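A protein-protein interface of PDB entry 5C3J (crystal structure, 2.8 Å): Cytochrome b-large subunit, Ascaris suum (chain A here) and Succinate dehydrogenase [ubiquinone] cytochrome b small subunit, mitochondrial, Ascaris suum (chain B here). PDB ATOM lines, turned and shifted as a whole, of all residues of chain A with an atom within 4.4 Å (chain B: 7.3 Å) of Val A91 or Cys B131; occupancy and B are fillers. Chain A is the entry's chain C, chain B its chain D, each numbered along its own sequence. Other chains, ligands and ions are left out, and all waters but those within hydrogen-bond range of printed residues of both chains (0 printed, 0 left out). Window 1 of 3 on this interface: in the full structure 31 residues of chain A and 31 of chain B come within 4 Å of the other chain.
The backbone carbonyl oxygen of Gly A90 sits close to the backbone carbonyl oxygen of Gly B135.
SG of Cys B131 sits at hydrogen-bond distance from O of Ile B127.
Leu A87 touches Phe B128 (CD2 to CE1, 3.2 Å).
Leu A87 touches Cys B131 (CD1 to C, 3.8 Å).
Leu B132 touches Leu A87 (N to CD1, 3.6 Å).
CG2 of Val A91 touches O of Cys B131 (3.7 Å).
Val A91 touches Gly B135.
Phe A93 touches Phe B139.
Tyr B138 touches Ser A94.
Gly A90 touches just one residue of chain B: Gly B135 (3.0 Å).
Val A91 touches just these residues of chain B: Cys B131 and Gly B135.
No residue of chain B comes within 4 Å of Gly A92.
Of the printed residues of chain B, Phe A93 touches Phe B139.
Of the printed residues of chain B, Ser A94 touches Tyr B138.
Val A95 touches none of the printed residues of chain B.
Of chain A, only Leu A87 (3.8 Å) and Val A91 (3.7 Å) come within 4 Å of Cys B131.
Of the printed residues of chain A, Leu B132 touches Leu A87 (3.6 Å).
Of the printed residues of chain A, Gly B135 touches Gly A90 and Val A91.
Leu B137 touches none of the printed residues of chain A.
Printed residues of chain A within 4 Å of Phe B139: Phe A93 (3.9 Å).
The nearest printed residue of chain A that does not touch Tyr B138 is Phe A93 (4.8 Å).
Hydrophobic or aromatic side chains of chain A that line the printed part of chain B: Leu A87, Val A91 and Phe A93.
Hydrophobic or aromatic side chains of chain B that line the printed part of chain A: Phe B128, Leu B132, Tyr B138 and Phe B139.
Among the printed residues, 8 pairs touch across the chains.
Among the printed residues, no Asp or Glu carboxylate lies within 4 Å of a Lys or Arg side-chain nitrogen of the other chain.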
ATOM      1  N   LEU A  87       8.161  -5.679   7.658  1.00  0.00           N
ATOM      2  CA  LEU A  87       7.262  -6.832   7.527  1.00  0.00           C
ATOM      3  C   LEU A  87       8.046  -8.075   7.106  1.00  0.00           C
ATOM      4  O   LEU A  87       7.897  -9.132   7.722  1.00  0.00           O
ATOM      5  CB  LEU A  87       6.124  -6.559   6.542  1.00  0.00           C
ATOM      6  CG  LEU A  87       5.028  -7.631   6.457  1.00  0.00           C
ATOM      7  CD1 LEU A  87       4.372  -7.859   7.816  1.00  0.00           C
ATOM      8  CD2 LEU A  87       3.981  -7.254   5.415  1.00  0.00           C
ATOM      9  N   ILE A  88       8.892  -7.939   6.081  1.00  0.00           N
ATOM     10  CA  ILE A  88       9.713  -9.063   5.603  1.00  0.00           C
ATOM     11  C   ILE A  88      10.700  -9.511   6.684  1.00  0.00           C
ATOM     12  O   ILE A  88      11.069 -10.679   6.729  1.00  0.00           O
ATOM     13  CB  ILE A  88      10.491  -8.731   4.297  1.00  0.00           C
ATOM     14  CG1 ILE A  88       9.538  -8.339   3.146  1.00  0.00           C
ATOM     15  CG2 ILE A  88      11.387  -9.897   3.880  1.00  0.00           C
ATOM     16  CD1 ILE A  88       8.485  -9.373   2.785  1.00  0.00           C
ATOM     17  N   GLY A  89      11.118  -8.583   7.546  1.00  0.00           N
ATOM     18  CA  GLY A  89      12.069  -8.875   8.622  1.00  0.00           C
ATOM     19  C   GLY A  89      11.387  -9.463   9.838  1.00  0.00           C
ATOM     20  O   GLY A  89      11.609 -10.619  10.182  1.00  0.00           O
ATOM     21  N   GLY A  90      10.542  -8.666  10.482  1.00  0.00           N
ATOM     22  CA  GLY A  90       9.805  -9.110  11.664  1.00  0.00           C
ATOM     23  C   GLY A  90       9.065 -10.432  11.499  1.00  0.00           C
ATOM     24  O   GLY A  90       8.918 -11.187  12.455  1.00  0.00           O
ATOM     25  N   VAL A  91       8.582 -10.713  10.294  1.00  0.00           N
ATOM     26  CA  VAL A  91       7.902 -11.982  10.029  1.00  0.00           C
ATOM     27  C   VAL A  91       8.897 -12.994   9.469  1.00  0.00           C
ATOM     28  O   VAL A  91       8.872 -14.155   9.859  1.00  0.00           O
ATOM     29  CB  VAL A  91       6.678 -11.794   9.097  1.00  0.00           C
ATOM     30  CG1 VAL A  91       6.156 -13.131   8.571  1.00  0.00           C
ATOM     31  CG2 VAL A  91       5.579 -11.031   9.835  1.00  0.00           C
ATOM     32  N   GLY A  92       9.771 -12.552   8.567  1.00  0.00           N
ATOM     33  CA  GLY A  92      10.867 -13.389   8.078  1.00  0.00           C
ATOM     34  C   GLY A  92      11.593 -14.103   9.206  1.00  0.00           C
ATOM     35  O   GLY A  92      11.475 -15.317   9.338  1.00  0.00           O
ATOM     36  N   PHE A  93      12.319 -13.360  10.042  1.00  0.00           N
ATOM     37  CA  PHE A  93      13.110 -13.984  11.113  1.00  0.00           C
ATOM     38  C   PHE A  93      12.254 -14.677  12.179  1.00  0.00           C
ATOM     39  O   PHE A  93      12.716 -15.609  12.848  1.00  0.00           O
ATOM     40  CB  PHE A  93      14.061 -12.971  11.753  1.00  0.00           C
ATOM     41  CG  PHE A  93      15.130 -12.471  10.809  1.00  0.00           C
ATOM     42  CD1 PHE A  93      15.083 -11.175  10.296  1.00  0.00           C
ATOM     43  CD2 PHE A  93      16.176 -13.305  10.419  1.00  0.00           C
ATOM     44  CE1 PHE A  93      16.055 -10.724   9.424  1.00  0.00           C
ATOM     45  CE2 PHE A  93      17.151 -12.857   9.545  1.00  0.00           C
ATOM     46  CZ  PHE A  93      17.090 -11.567   9.044  1.00  0.00           C
ATOM     47  N   SER A  94      11.010 -14.234  12.324  1.00  0.00           N
ATOM     48  CA  SER A  94      10.073 -14.896  13.225  1.00  0.00           C
ATOM     49  C   SER A  94       9.725 -16.279  12.705  1.00  0.00           C
ATOM     50  O   SER A  94       9.908 -17.272  13.389  1.00  0.00           O
ATOM     51  CB  SER A  94       8.786 -14.079  13.382  1.00  0.00           C
ATOM     52  OG  SER A  94       7.717 -14.888  13.858  1.00  0.00           O
ATOM     53  N   VAL A  95       9.214 -16.324  11.483  1.00  0.00           N
ATOM     54  CA  VAL A  95       8.697 -17.555  10.906  1.00  0.00           C
ATOM     55  C   VAL A  95       9.826 -18.532  10.533  1.00  0.00           C
ATOM     56  O   VAL A  95       9.639 -19.736  10.615  1.00  0.00           O
ATOM     57  CB  VAL A  95       7.746 -17.231   9.713  1.00  0.00           C
ATOM     58  CG1 VAL A  95       7.650 -18.376   8.707  1.00  0.00           C
ATOM     59  CG2 VAL A  95       6.357 -16.855  10.234  1.00  0.00           C
ATOM     60  N   ALA B 125      -4.875  -4.285   3.762  1.00  0.00           N
ATOM     61  CA  ALA B 125      -4.184  -3.249   4.528  1.00  0.00           C
ATOM     62  C   ALA B 125      -4.295  -3.510   6.028  1.00  0.00           C
ATOM     63  O   ALA B 125      -3.371  -3.203   6.784  1.00  0.00           O
ATOM     64  CB  ALA B 125      -4.742  -1.876   4.197  1.00  0.00           C
ATOM     65  N   TYR B 126      -5.422  -4.067   6.460  1.00  0.00           N
ATOM     66  CA  TYR B 126      -5.587  -4.429   7.866  1.00  0.00           C
ATOM     67  C   TYR B 126      -4.724  -5.640   8.238  1.00  0.00           C
ATOM     68  O   TYR B 126      -4.052  -5.609   9.264  1.00  0.00           O
ATOM     69  CB  TYR B 126      -7.070  -4.606   8.227  1.00  0.00           C
ATOM     70  CG  TYR B 126      -7.727  -3.255   8.442  1.00  0.00           C
ATOM     71  CD1 TYR B 126      -8.051  -2.425   7.363  1.00  0.00           C
ATOM     72  CD2 TYR B 126      -7.959  -2.771   9.724  1.00  0.00           C
ATOM     73  CE1 TYR B 126      -8.617  -1.171   7.565  1.00  0.00           C
ATOM     74  CE2 TYR B 126      -8.528  -1.524   9.933  1.00  0.00           C
ATOM     75  CZ  TYR B 126      -8.853  -0.729   8.856  1.00  0.00           C
ATOM     76  OH  TYR B 126      -9.416   0.503   9.092  1.00  0.00           O
ATOM     77  N   ILE B 127      -4.719  -6.665   7.383  1.00  0.00           N
ATOM     78  CA  ILE B 127      -3.796  -7.809   7.491  1.00  0.00           C
ATOM     79  C   ILE B 127      -2.339  -7.333   7.635  1.00  0.00           C
ATOM     80  O   ILE B 127      -1.581  -7.846   8.467  1.00  0.00           O
ATOM     81  CB  ILE B 127      -3.889  -8.745   6.240  1.00  0.00           C
ATOM     82  CG1 ILE B 127      -5.327  -9.287   6.016  1.00  0.00           C
ATOM     83  CG2 ILE B 127      -2.872  -9.884   6.298  1.00  0.00           C
ATOM     84  CD1 ILE B 127      -6.079  -9.726   7.255  1.00  0.00           C
ATOM     85  N   PHE B 128      -1.960  -6.348   6.822  1.00  0.00           N
ATOM     86  CA  PHE B 128      -0.592  -5.793   6.819  1.00  0.00           C
ATOM     87  C   PHE B 128      -0.205  -5.224   8.191  1.00  0.00           C
ATOM     88  O   PHE B 128       0.831  -5.567   8.741  1.00  0.00           O
ATOM     89  CB  PHE B 128      -0.460  -4.701   5.739  1.00  0.00           C
ATOM     90  CG  PHE B 128       0.952  -4.273   5.476  1.00  0.00           C
ATOM     91  CD1 PHE B 128       1.673  -4.824   4.431  1.00  0.00           C
ATOM     92  CD2 PHE B 128       1.560  -3.321   6.271  1.00  0.00           C
ATOM     93  CE1 PHE B 128       2.979  -4.427   4.175  1.00  0.00           C
ATOM     94  CE2 PHE B 128       2.867  -2.921   6.030  1.00  0.00           C
ATOM     95  CZ  PHE B 128       3.579  -3.471   4.976  1.00  0.00           C
ATOM     96  N   THR B 129      -1.047  -4.350   8.726  1.00  0.00           N
ATOM     97  CA  THR B 129      -0.821  -3.764  10.037  1.00  0.00           C
ATOM     98  C   THR B 129      -0.700  -4.857  11.105  1.00  0.00           C
ATOM     99  O   THR B 129       0.284  -4.918  11.842  1.00  0.00           O
ATOM    100  CB  THR B 129      -1.968  -2.797  10.392  1.00  0.00           C
ATOM    101  OG1 THR B 129      -1.980  -1.715   9.449  1.00  0.00           O
ATOM    102  CG2 THR B 129      -1.814  -2.235  11.790  1.00  0.00           C
ATOM    103  N   ALA B 130      -1.698  -5.729  11.165  1.00  0.00           N
ATOM    104  CA  ALA B 130      -1.736  -6.789  12.168  1.00  0.00           C
ATOM    105  C   ALA B 130      -0.533  -7.734  12.104  1.00  0.00           C
ATOM    106  O   ALA B 130       0.010  -8.126  13.133  1.00  0.00           O
ATOM    107  CB  ALA B 130      -3.027  -7.581  12.036  1.00  0.00           C
ATOM    108  N   CYS B 131      -0.125  -8.111  10.903  1.00  0.00           N
ATOM    109  CA  CYS B 131       1.031  -8.995  10.756  1.00  0.00           C
ATOM    110  C   CYS B 131       2.342  -8.261  11.054  1.00  0.00           C
ATOM    111  O   CYS B 131       3.262  -8.844  11.628  1.00  0.00           O
ATOM    112  CB  CYS B 131       1.040  -9.641   9.368  1.00  0.00           C
ATOM    113  SG  CYS B 131      -0.427 -10.679   9.103  1.00  0.00           S
ATOM    114  N   LEU B 132       2.407  -6.984  10.685  1.00  0.00           N
ATOM    115  CA  LEU B 132       3.553  -6.144  11.005  1.00  0.00           C
ATOM    116  C   LEU B 132       3.806  -6.113  12.508  1.00  0.00           C
ATOM    117  O   LEU B 132       4.932  -6.327  12.953  1.00  0.00           O
ATOM    118  CB  LEU B 132       3.329  -4.717  10.496  1.00  0.00           C
ATOM    119  CG  LEU B 132       4.427  -3.684  10.791  1.00  0.00           C
ATOM    120  CD1 LEU B 132       5.714  -3.980  10.024  1.00  0.00           C
ATOM    121  CD2 LEU B 132       3.924  -2.284  10.479  1.00  0.00           C
ATOM    122  N   LEU B 133       2.759  -5.838  13.283  1.00  0.00           N
ATOM    123  CA  LEU B 133       2.880  -5.826  14.742  1.00  0.00           C
ATOM    124  C   LEU B 133       3.309  -7.200  15.254  1.00  0.00           C
ATOM    125  O   LEU B 133       4.318  -7.325  15.951  1.00  0.00           O
ATOM    126  CB  LEU B 133       1.570  -5.411  15.440  1.00  0.00           C
ATOM    127  CG  LEU B 133       1.711  -5.279  16.972  1.00  0.00           C
ATOM    128  CD1 LEU B 133       2.630  -4.117  17.326  1.00  0.00           C
ATOM    129  CD2 LEU B 133       0.379  -5.140  17.700  1.00  0.00           C
ATOM    130  N   ALA B 134       2.546  -8.228  14.905  1.00  0.00           N
ATOM    131  CA  ALA B 134       2.826  -9.566  15.406  1.00  0.00           C
ATOM    132  C   ALA B 134       4.274  -9.962  15.114  1.00  0.00           C
ATOM    133  O   ALA B 134       4.943 -10.519  15.978  1.00  0.00           O
ATOM    134  CB  ALA B 134       1.843 -10.584  14.833  1.00  0.00           C
ATOM    135  N   GLY B 135       4.752  -9.647  13.912  1.00  0.00           N
ATOM    136  CA  GLY B 135       6.157  -9.840  13.560  1.00  0.00           C
ATOM    137  C   GLY B 135       7.119  -8.972  14.361  1.00  0.00           C
ATOM    138  O   GLY B 135       8.199  -9.419  14.735  1.00  0.00           O
ATOM    139  N   LEU B 136       6.752  -7.724  14.623  1.00  0.00           N
ATOM    140  CA  LEU B 136       7.604  -6.857  15.446  1.00  0.00           C
ATOM    141  C   LEU B 136       7.636  -7.315  16.905  1.00  0.00           C
ATOM    142  O   LEU B 136       8.709  -7.510  17.470  1.00  0.00           O
ATOM    143  CB  LEU B 136       7.174  -5.388  15.345  1.00  0.00           C
ATOM    144  CG  LEU B 136       7.929  -4.537  14.315  1.00  0.00           C
ATOM    145  CD1 LEU B 136       8.203  -5.297  13.026  1.00  0.00           C
ATOM    146  CD2 LEU B 136       7.156  -3.255  14.028  1.00  0.00           C
ATOM    147  N   LEU B 137       6.467  -7.496  17.512  1.00  0.00           N
ATOM    148  CA  LEU B 137       6.403  -8.034  18.862  1.00  0.00           C
ATOM    149  C   LEU B 137       7.250  -9.303  18.979  1.00  0.00           C
ATOM    150  O   LEU B 137       8.049  -9.423  19.895  1.00  0.00           O
ATOM    151  CB  LEU B 137       4.964  -8.327  19.278  1.00  0.00           C
ATOM    152  CG  LEU B 137       4.073  -7.098  19.477  1.00  0.00           C
ATOM    153  CD1 LEU B 137       2.653  -7.521  19.829  1.00  0.00           C
ATOM    154  CD2 LEU B 137       4.630  -6.153  20.535  1.00  0.00           C
ATOM    155  N   TYR B 138       7.099 -10.236  18.046  1.00  0.00           N
ATOM    156  CA  TYR B 138       7.857 -11.481  18.116  1.00  0.00           C
ATOM    157  C   TYR B 138       9.354 -11.221  18.185  1.00  0.00           C
ATOM    158  O   TYR B 138      10.047 -11.819  19.002  1.00  0.00           O
ATOM    159  CB  TYR B 138       7.575 -12.377  16.915  1.00  0.00           C
ATOM    160  CG  TYR B 138       8.213 -13.737  17.037  1.00  0.00           C
ATOM    161  CD1 TYR B 138       9.563 -13.935  16.715  1.00  0.00           C
ATOM    162  CD2 TYR B 138       7.471 -14.831  17.483  1.00  0.00           C
ATOM    163  CE1 TYR B 138      10.151 -15.189  16.834  1.00  0.00           C
ATOM    164  CE2 TYR B 138       8.045 -16.091  17.603  1.00  0.00           C
ATOM    165  CZ  TYR B 138       9.384 -16.269  17.278  1.00  0.00           C
ATOM    166  OH  TYR B 138       9.946 -17.523  17.400  1.00  0.00           O
ATOM    167  N   PHE B 139       9.839 -10.336  17.318  1.00  0.00           N
ATOM    168  CA  PHE B 139      11.277 -10.063  17.166  1.00  0.00           C
ATOM    169  C   PHE B 139      11.864  -9.390  18.411  1.00  0.00           C
ATOM    170  O   PHE B 139      12.969  -9.720  18.841  1.00  0.00           O
ATOM    171  CB  PHE B 139      11.486  -9.192  15.927  1.00  0.00           C
ATOM    172  CG  PHE B 139      12.906  -9.101  15.465  1.00  0.00           C
ATOM    173  CD1 PHE B 139      13.453 -10.098  14.661  1.00  0.00           C
ATOM    174  CD2 PHE B 139      13.686  -7.995  15.789  1.00  0.00           C
ATOM    175  CE1 PHE B 139      14.763 -10.011  14.207  1.00  0.00           C
ATOM    176  CE2 PHE B 139      14.998  -7.900  15.341  1.00  0.00           C
ATOM    177  CZ  PHE B 139      15.539  -8.910  14.549  1.00  0.00           C
